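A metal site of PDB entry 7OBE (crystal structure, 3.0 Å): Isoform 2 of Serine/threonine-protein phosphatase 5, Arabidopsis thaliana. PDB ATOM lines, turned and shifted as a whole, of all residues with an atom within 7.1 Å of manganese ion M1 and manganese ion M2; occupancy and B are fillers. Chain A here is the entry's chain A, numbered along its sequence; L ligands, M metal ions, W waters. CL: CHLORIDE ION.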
ATOM      1  N   GLU A  81     -12.284 -22.581   1.861  1.00  0.00           N
ATOM      2  CA  GLU A  81     -13.724 -22.339   1.979  1.00  0.00           C
ATOM      3  C   GLU A  81     -14.296 -22.889   3.284  1.00  0.00           C
ATOM      4  O   GLU A  81     -15.505 -23.146   3.370  1.00  0.00           O
ATOM      5  CB  GLU A  81     -14.486 -22.906   0.782  1.00  0.00           C
ATOM      6  CG  GLU A  81     -14.345 -22.086  -0.482  1.00  0.00           C
ATOM      7  CD  GLU A  81     -14.527 -22.932  -1.726  1.00  0.00           C
ATOM      8  OE1 GLU A  81     -15.334 -23.883  -1.700  1.00  0.00           O
ATOM      9  OE2 GLU A  81     -13.832 -22.655  -2.737  1.00  0.00           O
ATOM     10  N   ASP A 248     -17.408 -31.720  -8.701  1.00  0.00           N
ATOM     11  CA  ASP A 248     -17.529 -30.296  -8.978  1.00  0.00           C
ATOM     12  C   ASP A 248     -16.761 -29.923 -10.239  1.00  0.00           C
ATOM     13  O   ASP A 248     -15.637 -30.395 -10.462  1.00  0.00           O
ATOM     14  CB  ASP A 248     -17.000 -29.485  -7.798  1.00  0.00           C
ATOM     15  CG  ASP A 248     -17.854 -29.644  -6.560  1.00  0.00           C
ATOM     16  OD1 ASP A 248     -18.457 -30.722  -6.407  1.00  0.00           O
ATOM     17  OD2 ASP A 248     -17.890 -28.717  -5.729  1.00  0.00           O
ATOM     18  N   VAL A 249     -17.368 -29.084 -11.075  1.00  0.00           N
ATOM     19  CA  VAL A 249     -16.662 -28.493 -12.199  1.00  0.00           C
ATOM     20  C   VAL A 249     -16.631 -26.981 -12.154  1.00  0.00           C
ATOM     21  O   VAL A 249     -15.769 -26.375 -12.815  1.00  0.00           O
ATOM     22  CB  VAL A 249     -17.236 -28.980 -13.550  1.00  0.00           C
ATOM     23  CG1 VAL A 249     -16.918 -30.452 -13.756  1.00  0.00           C
ATOM     24  CG2 VAL A 249     -18.730 -28.737 -13.599  1.00  0.00           C
ATOM     25  N   HIS A 250     -17.528 -26.346 -11.392  1.00  0.00           N
ATOM     26  CA  HIS A 250     -17.527 -24.913 -11.105  1.00  0.00           C
ATOM     27  C   HIS A 250     -17.127 -24.064 -12.314  1.00  0.00           C
ATOM     28  O   HIS A 250     -16.190 -23.286 -12.287  1.00  0.00           O
ATOM     29  CB  HIS A 250     -16.629 -24.598  -9.910  1.00  0.00           C
ATOM     30  CG  HIS A 250     -17.198 -24.996  -8.587  1.00  0.00           C
ATOM     31  ND1 HIS A 250     -18.272 -24.355  -8.009  1.00  0.00           N
ATOM     32  CD2 HIS A 250     -16.832 -25.969  -7.705  1.00  0.00           C
ATOM     33  CE1 HIS A 250     -18.555 -24.918  -6.857  1.00  0.00           C
ATOM     34  NE2 HIS A 250     -17.699 -25.896  -6.643  1.00  0.00           N
ATOM     35  N   ASN A 275     -22.236 -34.565 -10.243  1.00  0.00           N
ATOM     36  CA  ASN A 275     -22.688 -34.494  -8.847  1.00  0.00           C
ATOM     37  C   ASN A 275     -22.722 -33.050  -8.350  1.00  0.00           C
ATOM     38  O   ASN A 275     -22.069 -32.673  -7.374  1.00  0.00           O
ATOM     39  CB  ASN A 275     -21.807 -35.372  -7.972  1.00  0.00           C
ATOM     40  CG  ASN A 275     -22.478 -35.802  -6.682  1.00  0.00           C
ATOM     41  OD1 ASN A 275     -23.708 -35.847  -6.590  1.00  0.00           O
ATOM     42  ND2 ASN A 275     -21.678 -36.131  -5.682  1.00  0.00           N
ATOM     43  N   GLY A 276     -23.495 -32.227  -9.056  1.00  0.00           N
ATOM     44  CA  GLY A 276     -23.757 -30.863  -8.630  1.00  0.00           C
ATOM     45  C   GLY A 276     -22.564 -29.942  -8.791  1.00  0.00           C
ATOM     46  O   GLY A 276     -21.478 -30.326  -9.210  1.00  0.00           O
ATOM     47  N   ASP A 277     -22.800 -28.680  -8.434  1.00  0.00           N
ATOM     48  CA  ASP A 277     -21.811 -27.615  -8.493  1.00  0.00           C
ATOM     49  C   ASP A 277     -21.208 -27.503  -9.887  1.00  0.00           C
ATOM     50  O   ASP A 277     -19.997 -27.617 -10.096  1.00  0.00           O
ATOM     51  CB  ASP A 277     -20.723 -27.823  -7.434  1.00  0.00           C
ATOM     52  CG  ASP A 277     -21.068 -27.164  -6.109  1.00  0.00           C
ATOM     53  OD1 ASP A 277     -22.240 -26.773  -5.935  1.00  0.00           O
ATOM     54  OD2 ASP A 277     -20.172 -27.019  -5.251  1.00  0.00           O
ATOM     55  N   VAL A 279     -21.714 -24.695 -11.716  1.00  0.00           N
ATOM     56  CA  VAL A 279     -21.519 -23.288 -12.008  1.00  0.00           C
ATOM     57  C   VAL A 279     -20.835 -22.580 -10.838  1.00  0.00           C
ATOM     58  O   VAL A 279     -20.349 -23.240  -9.908  1.00  0.00           O
ATOM     59  CB  VAL A 279     -22.863 -22.611 -12.354  1.00  0.00           C
ATOM     60  CG1 VAL A 279     -23.519 -23.320 -13.531  1.00  0.00           C
ATOM     61  CG2 VAL A 279     -23.776 -22.645 -11.136  1.00  0.00           C
ATOM     62  N   ARG A 281     -17.941 -19.619  -9.260  1.00  0.00           N
ATOM     63  CA  ARG A 281     -16.505 -19.688  -8.979  1.00  0.00           C
ATOM     64  C   ARG A 281     -15.689 -19.623 -10.264  1.00  0.00           C
ATOM     65  O   ARG A 281     -14.823 -18.757 -10.402  1.00  0.00           O
ATOM     66  CB  ARG A 281     -16.193 -20.954  -8.183  1.00  0.00           C
ATOM     67  CG  ARG A 281     -15.013 -20.823  -7.242  1.00  0.00           C
ATOM     68  CD  ARG A 281     -15.344 -20.028  -5.989  1.00  0.00           C
ATOM     69  NE  ARG A 281     -16.071 -20.809  -5.003  1.00  0.00           N
ATOM     70  CZ  ARG A 281     -16.182 -20.465  -3.726  1.00  0.00           C
ATOM     71  NH1 ARG A 281     -15.586 -19.372  -3.268  1.00  0.00           N
ATOM     72  NH2 ARG A 281     -16.869 -21.234  -2.881  1.00  0.00           N
ATOM     73  N   GLY A 308     -26.041 -29.317  -6.469  1.00  0.00           N
ATOM     74  CA  GLY A 308     -25.046 -28.910  -5.506  1.00  0.00           C
ATOM     75  C   GLY A 308     -25.514 -27.719  -4.683  1.00  0.00           C
ATOM     76  O   GLY A 308     -26.614 -27.206  -4.841  1.00  0.00           O
ATOM     77  N   ASN A 309     -24.632 -27.283  -3.783  1.00  0.00           N
ATOM     78  CA  ASN A 309     -24.950 -26.110  -2.986  1.00  0.00           C
ATOM     79  C   ASN A 309     -24.876 -24.834  -3.809  1.00  0.00           C
ATOM     80  O   ASN A 309     -25.536 -23.852  -3.461  1.00  0.00           O
ATOM     81  CB  ASN A 309     -24.019 -26.018  -1.783  1.00  0.00           C
ATOM     82  CG  ASN A 309     -22.573 -26.254  -2.154  1.00  0.00           C
ATOM     83  OD1 ASN A 309     -22.244 -27.279  -2.753  1.00  0.00           O
ATOM     84  ND2 ASN A 309     -21.702 -25.324  -1.782  1.00  0.00           N
ATOM     85  N   HIS A 310     -24.111 -24.826  -4.906  1.00  0.00           N
ATOM     86  CA  HIS A 310     -23.932 -23.646  -5.735  1.00  0.00           C
ATOM     87  C   HIS A 310     -24.963 -23.560  -6.857  1.00  0.00           C
ATOM     88  O   HIS A 310     -24.862 -22.661  -7.702  1.00  0.00           O
ATOM     89  CB  HIS A 310     -22.519 -23.624  -6.321  1.00  0.00           C
ATOM     90  CG  HIS A 310     -21.521 -22.981  -5.417  1.00  0.00           C
ATOM     91  ND1 HIS A 310     -21.377 -21.609  -5.309  1.00  0.00           N
ATOM     92  CD2 HIS A 310     -20.611 -23.518  -4.569  1.00  0.00           C
ATOM     93  CE1 HIS A 310     -20.426 -21.334  -4.441  1.00  0.00           C
ATOM     94  NE2 HIS A 310     -19.948 -22.476  -3.971  1.00  0.00           N
ATOM     95  N   HIS A 358     -24.195 -34.908  -3.250  1.00  0.00           N
ATOM     96  CA  HIS A 358     -23.137 -33.919  -3.419  1.00  0.00           C
ATOM     97  C   HIS A 358     -22.428 -33.637  -2.098  1.00  0.00           C
ATOM     98  O   HIS A 358     -21.197 -33.743  -2.020  1.00  0.00           O
ATOM     99  CB  HIS A 358     -23.724 -32.630  -3.993  1.00  0.00           C
ATOM    100  CG  HIS A 358     -22.738 -31.505  -4.075  1.00  0.00           C
ATOM    101  ND1 HIS A 358     -21.817 -31.404  -5.102  1.00  0.00           N
ATOM    102  CD2 HIS A 358     -22.525 -30.450  -3.268  1.00  0.00           C
ATOM    103  CE1 HIS A 358     -21.083 -30.314  -4.914  1.00  0.00           C
ATOM    104  NE2 HIS A 358     -21.497 -29.726  -3.816  1.00  0.00           N
ATOM    105  N   GLY A 359     -23.182 -33.298  -1.056  1.00  0.00           N
ATOM    106  CA  GLY A 359     -22.598 -32.952   0.226  1.00  0.00           C
ATOM    107  C   GLY A 359     -22.292 -34.144   1.094  1.00  0.00           C
ATOM    108  O   GLY A 359     -21.129 -34.479   1.307  1.00  0.00           O
ATOM    109  N   LEU A 391     -26.677 -31.351   1.023  1.00  0.00           N
ATOM    110  CA  LEU A 391     -26.047 -30.457   0.067  1.00  0.00           C
ATOM    111  C   LEU A 391     -24.798 -29.771   0.600  1.00  0.00           C
ATOM    112  O   LEU A 391     -24.018 -29.243  -0.200  1.00  0.00           O
ATOM    113  CB  LEU A 391     -27.043 -29.383  -0.388  1.00  0.00           C
ATOM    114  CG  LEU A 391     -28.048 -29.794  -1.460  1.00  0.00           C
ATOM    115  CD1 LEU A 391     -29.046 -28.684  -1.698  1.00  0.00           C
ATOM    116  CD2 LEU A 391     -27.321 -30.135  -2.745  1.00  0.00           C
ATOM    117  N   TRP A 392     -24.582 -29.774   1.922  1.00  0.00           N
ATOM    118  CA  TRP A 392     -23.520 -28.983   2.526  1.00  0.00           C
ATOM    119  C   TRP A 392     -22.575 -29.772   3.428  1.00  0.00           C
ATOM    120  O   TRP A 392     -21.551 -29.213   3.827  1.00  0.00           O
ATOM    121  CB  TRP A 392     -24.128 -27.832   3.350  1.00  0.00           C
ATOM    122  CG  TRP A 392     -24.544 -26.661   2.531  1.00  0.00           C
ATOM    123  CD1 TRP A 392     -25.763 -26.451   1.959  1.00  0.00           C
ATOM    124  CD2 TRP A 392     -23.742 -25.522   2.189  1.00  0.00           C
ATOM    125  NE1 TRP A 392     -25.770 -25.251   1.277  1.00  0.00           N
ATOM    126  CE2 TRP A 392     -24.542 -24.662   1.404  1.00  0.00           C
ATOM    127  CE3 TRP A 392     -22.419 -25.148   2.465  1.00  0.00           C
ATOM    128  CZ2 TRP A 392     -24.060 -23.458   0.899  1.00  0.00           C
ATOM    129  CZ3 TRP A 392     -21.953 -23.948   1.965  1.00  0.00           C
ATOM    130  CH2 TRP A 392     -22.774 -23.123   1.187  1.00  0.00           C
ATOM    131  N   ARG A 406     -17.622 -25.380   7.446  1.00  0.00           N
ATOM    132  CA  ARG A 406     -18.149 -24.334   6.577  1.00  0.00           C
ATOM    133  C   ARG A 406     -19.173 -23.436   7.259  1.00  0.00           C
ATOM    134  O   ARG A 406     -19.651 -22.471   6.643  1.00  0.00           O
ATOM    135  CB  ARG A 406     -18.784 -24.952   5.331  1.00  0.00           C
ATOM    136  CG  ARG A 406     -17.943 -26.017   4.659  1.00  0.00           C
ATOM    137  CD  ARG A 406     -18.375 -26.219   3.215  1.00  0.00           C
ATOM    138  NE  ARG A 406     -17.837 -27.461   2.654  1.00  0.00           N
ATOM    139  CZ  ARG A 406     -17.208 -27.541   1.495  1.00  0.00           C
ATOM    140  NH1 ARG A 406     -16.752 -28.707   1.062  1.00  0.00           N
ATOM    141  NH2 ARG A 406     -17.037 -26.449   0.753  1.00  0.00           N
ATOM    142  N   SER A 432     -18.997 -35.176  -3.412  1.00  0.00           N
ATOM    143  CA  SER A 432     -18.051 -34.187  -3.931  1.00  0.00           C
ATOM    144  C   SER A 432     -17.882 -33.033  -2.958  1.00  0.00           C
ATOM    145  O   SER A 432     -17.417 -33.229  -1.827  1.00  0.00           O
ATOM    146  CB  SER A 432     -18.501 -33.704  -5.304  1.00  0.00           C
ATOM    147  OG  SER A 432     -18.637 -34.811  -6.177  1.00  0.00           O
ATOM    148  N   HIS A 433     -18.209 -31.812  -3.406  1.00  0.00           N
ATOM    149  CA  HIS A 433     -18.380 -30.648  -2.523  1.00  0.00           C
ATOM    150  C   HIS A 433     -17.073 -30.120  -1.938  1.00  0.00           C
ATOM    151  O   HIS A 433     -16.996 -28.938  -1.585  1.00  0.00           O
ATOM    152  CB  HIS A 433     -19.365 -30.996  -1.403  1.00  0.00           C
ATOM    153  CG  HIS A 433     -19.719 -29.846  -0.523  1.00  0.00           C
ATOM    154  ND1 HIS A 433     -20.132 -28.626  -1.024  1.00  0.00           N
ATOM    155  CD2 HIS A 433     -19.768 -29.734   0.826  1.00  0.00           C
ATOM    156  CE1 HIS A 433     -20.389 -27.812  -0.014  1.00  0.00           C
ATOM    157  NE2 HIS A 433     -20.177 -28.457   1.118  1.00  0.00           N
ATOM    158  N   GLU A 434     -16.049 -30.971  -1.825  1.00  0.00           N
ATOM    159  CA  GLU A 434     -14.788 -30.626  -1.200  1.00  0.00           C
ATOM    160  C   GLU A 434     -13.641 -30.816  -2.188  1.00  0.00           C
ATOM    161  O   GLU A 434     -13.566 -31.828  -2.876  1.00  0.00           O
ATOM    162  CB  GLU A 434     -14.530 -31.481   0.047  1.00  0.00           C
ATOM    163  CG  GLU A 434     -13.949 -30.732   1.232  1.00  0.00           C
ATOM    164  CD  GLU A 434     -13.902 -31.582   2.501  1.00  0.00           C
ATOM    165  OE1 GLU A 434     -13.677 -31.011   3.592  1.00  0.00           O
ATOM    166  OE2 GLU A 434     -14.087 -32.813   2.401  1.00  0.00           O
ATOM    167  N   VAL A 435     -12.743 -29.825  -2.233  1.00  0.00           N
ATOM    168  CA  VAL A 435     -11.578 -29.913  -3.111  1.00  0.00           C
ATOM    169  C   VAL A 435     -10.608 -30.954  -2.560  1.00  0.00           C
ATOM    170  O   VAL A 435     -10.465 -31.117  -1.349  1.00  0.00           O
ATOM    171  CB  VAL A 435     -10.921 -28.521  -3.244  1.00  0.00           C
ATOM    172  CG1 VAL A 435     -10.526 -27.986  -1.877  1.00  0.00           C
ATOM    173  CG2 VAL A 435      -9.718 -28.573  -4.172  1.00  0.00           C
ATOM    174  N   PHE A 452     -13.852 -35.004  -7.351  1.00  0.00           N
ATOM    175  CA  PHE A 452     -13.786 -33.562  -7.613  1.00  0.00           C
ATOM    176  C   PHE A 452     -13.155 -33.372  -8.984  1.00  0.00           C
ATOM    177  O   PHE A 452     -11.990 -33.735  -9.179  1.00  0.00           O
ATOM    178  CB  PHE A 452     -12.992 -32.863  -6.514  1.00  0.00           C
ATOM    179  CG  PHE A 452     -13.014 -31.365  -6.587  1.00  0.00           C
ATOM    180  CD1 PHE A 452     -12.113 -30.675  -7.380  1.00  0.00           C
ATOM    181  CD2 PHE A 452     -13.929 -30.638  -5.839  1.00  0.00           C
ATOM    182  CE1 PHE A 452     -12.122 -29.299  -7.438  1.00  0.00           C
ATOM    183  CE2 PHE A 452     -13.943 -29.258  -5.889  1.00  0.00           C
ATOM    184  CZ  PHE A 452     -13.044 -28.591  -6.683  1.00  0.00           C
ATOM    185  N   TYR A 457      -8.199 -25.810  -9.211  1.00  0.00           N
ATOM    186  CA  TYR A 457      -9.372 -25.067  -8.757  1.00  0.00           C
ATOM    187  C   TYR A 457      -9.065 -23.581  -8.639  1.00  0.00           C
ATOM    188  O   TYR A 457      -8.038 -23.186  -8.073  1.00  0.00           O
ATOM    189  CB  TYR A 457      -9.828 -25.630  -7.409  1.00  0.00           C
ATOM    190  CG  TYR A 457     -11.157 -25.117  -6.904  1.00  0.00           C
ATOM    191  CD1 TYR A 457     -12.249 -24.988  -7.758  1.00  0.00           C
ATOM    192  CD2 TYR A 457     -11.325 -24.785  -5.563  1.00  0.00           C
ATOM    193  CE1 TYR A 457     -13.476 -24.534  -7.285  1.00  0.00           C
ATOM    194  CE2 TYR A 457     -12.541 -24.322  -5.087  1.00  0.00           C
ATOM    195  CZ  TYR A 457     -13.615 -24.203  -5.950  1.00  0.00           C
ATOM    196  OH  TYR A 457     -14.817 -23.746  -5.477  1.00  0.00           O
HETATM  197 CL    CL L   1     -18.914 -25.980  -2.665  1.00  0.00          CL
HETATM  198 MN    MN M   1     -20.334 -28.109  -3.189  1.00  0.00          MN
HETATM  199 MN    MN M   2     -17.868 -27.140  -4.732  1.00  0.00          MN
HETATM  200  O   HOH W   1     -15.799 -26.226  -4.222  1.00  0.00           O
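O of His 358 is in hydrogen-bond range of N of Ser 432 (3.0 Å). The guanidinium group (NH1) of Arg 406 lies within hydrogen-bond range of the backbone carbonyl oxygen (O) of His 433 (2.7 Å). OD1 of Asp 248 lies within hydrogen-bond range of N of His 433, at 3.2 Å. The backbone carbonyl oxygen (O) of Asn 275 is in hydrogen-bond range of a ring nitrogen (ND1) of His 358 (2.6 Å). The backbone carbonyl oxygen (O) of Trp 392 lies within hydrogen-bond range of a ring nitrogen (NE2) of His 433 (3.1 Å). The side-chain carboxylate of Asp 277 sits at hydrogen-bond distance from the backbone NH of His 310. A ring nitrogen (ND1) of His 250 lies within hydrogen-bond range of the backbone carbonyl oxygen (O) of Val 279 (3.0 Å). O of Asp 277 lies within hydrogen-bond range of N of Val 249, at 3.2 Å.
The nearest printed residue that does not touch manganese ion M1 is His 310 (4.8 Å).
Within 4 Å of manganese ion M2: Asp 248, His 250, Asp 277 and His 433.
NE2 of His 358 binds manganese ion M1. OD1 of Asn 309 binds manganese ion M1, 2.1 Å away. ND1 of His 433 binds manganese ion M1, at 2.2 Å. OD2 of Asp 277 is bound to manganese ion M1, 2.3 Å away. Manganese ion M1 is bound by CL of the ligand.
Manganese ion M2 is bound by the side-chain carboxylate (OD2) of Asp 248 (1.9 Å), a ring nitrogen (NE2) of His 250 (2.3 Å), water W1 (2.3 Å), the side-chain carboxylate (OD2) of Asp 277 (2.4 Å) and a chlorine (CL) of the ligand (2.6 Å).
Water W1 bridges the side-chain hydroxyl of Tyr 457 (2.9 Å) and the side-chain carboxylate of Glu 81 (3.5 Å).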
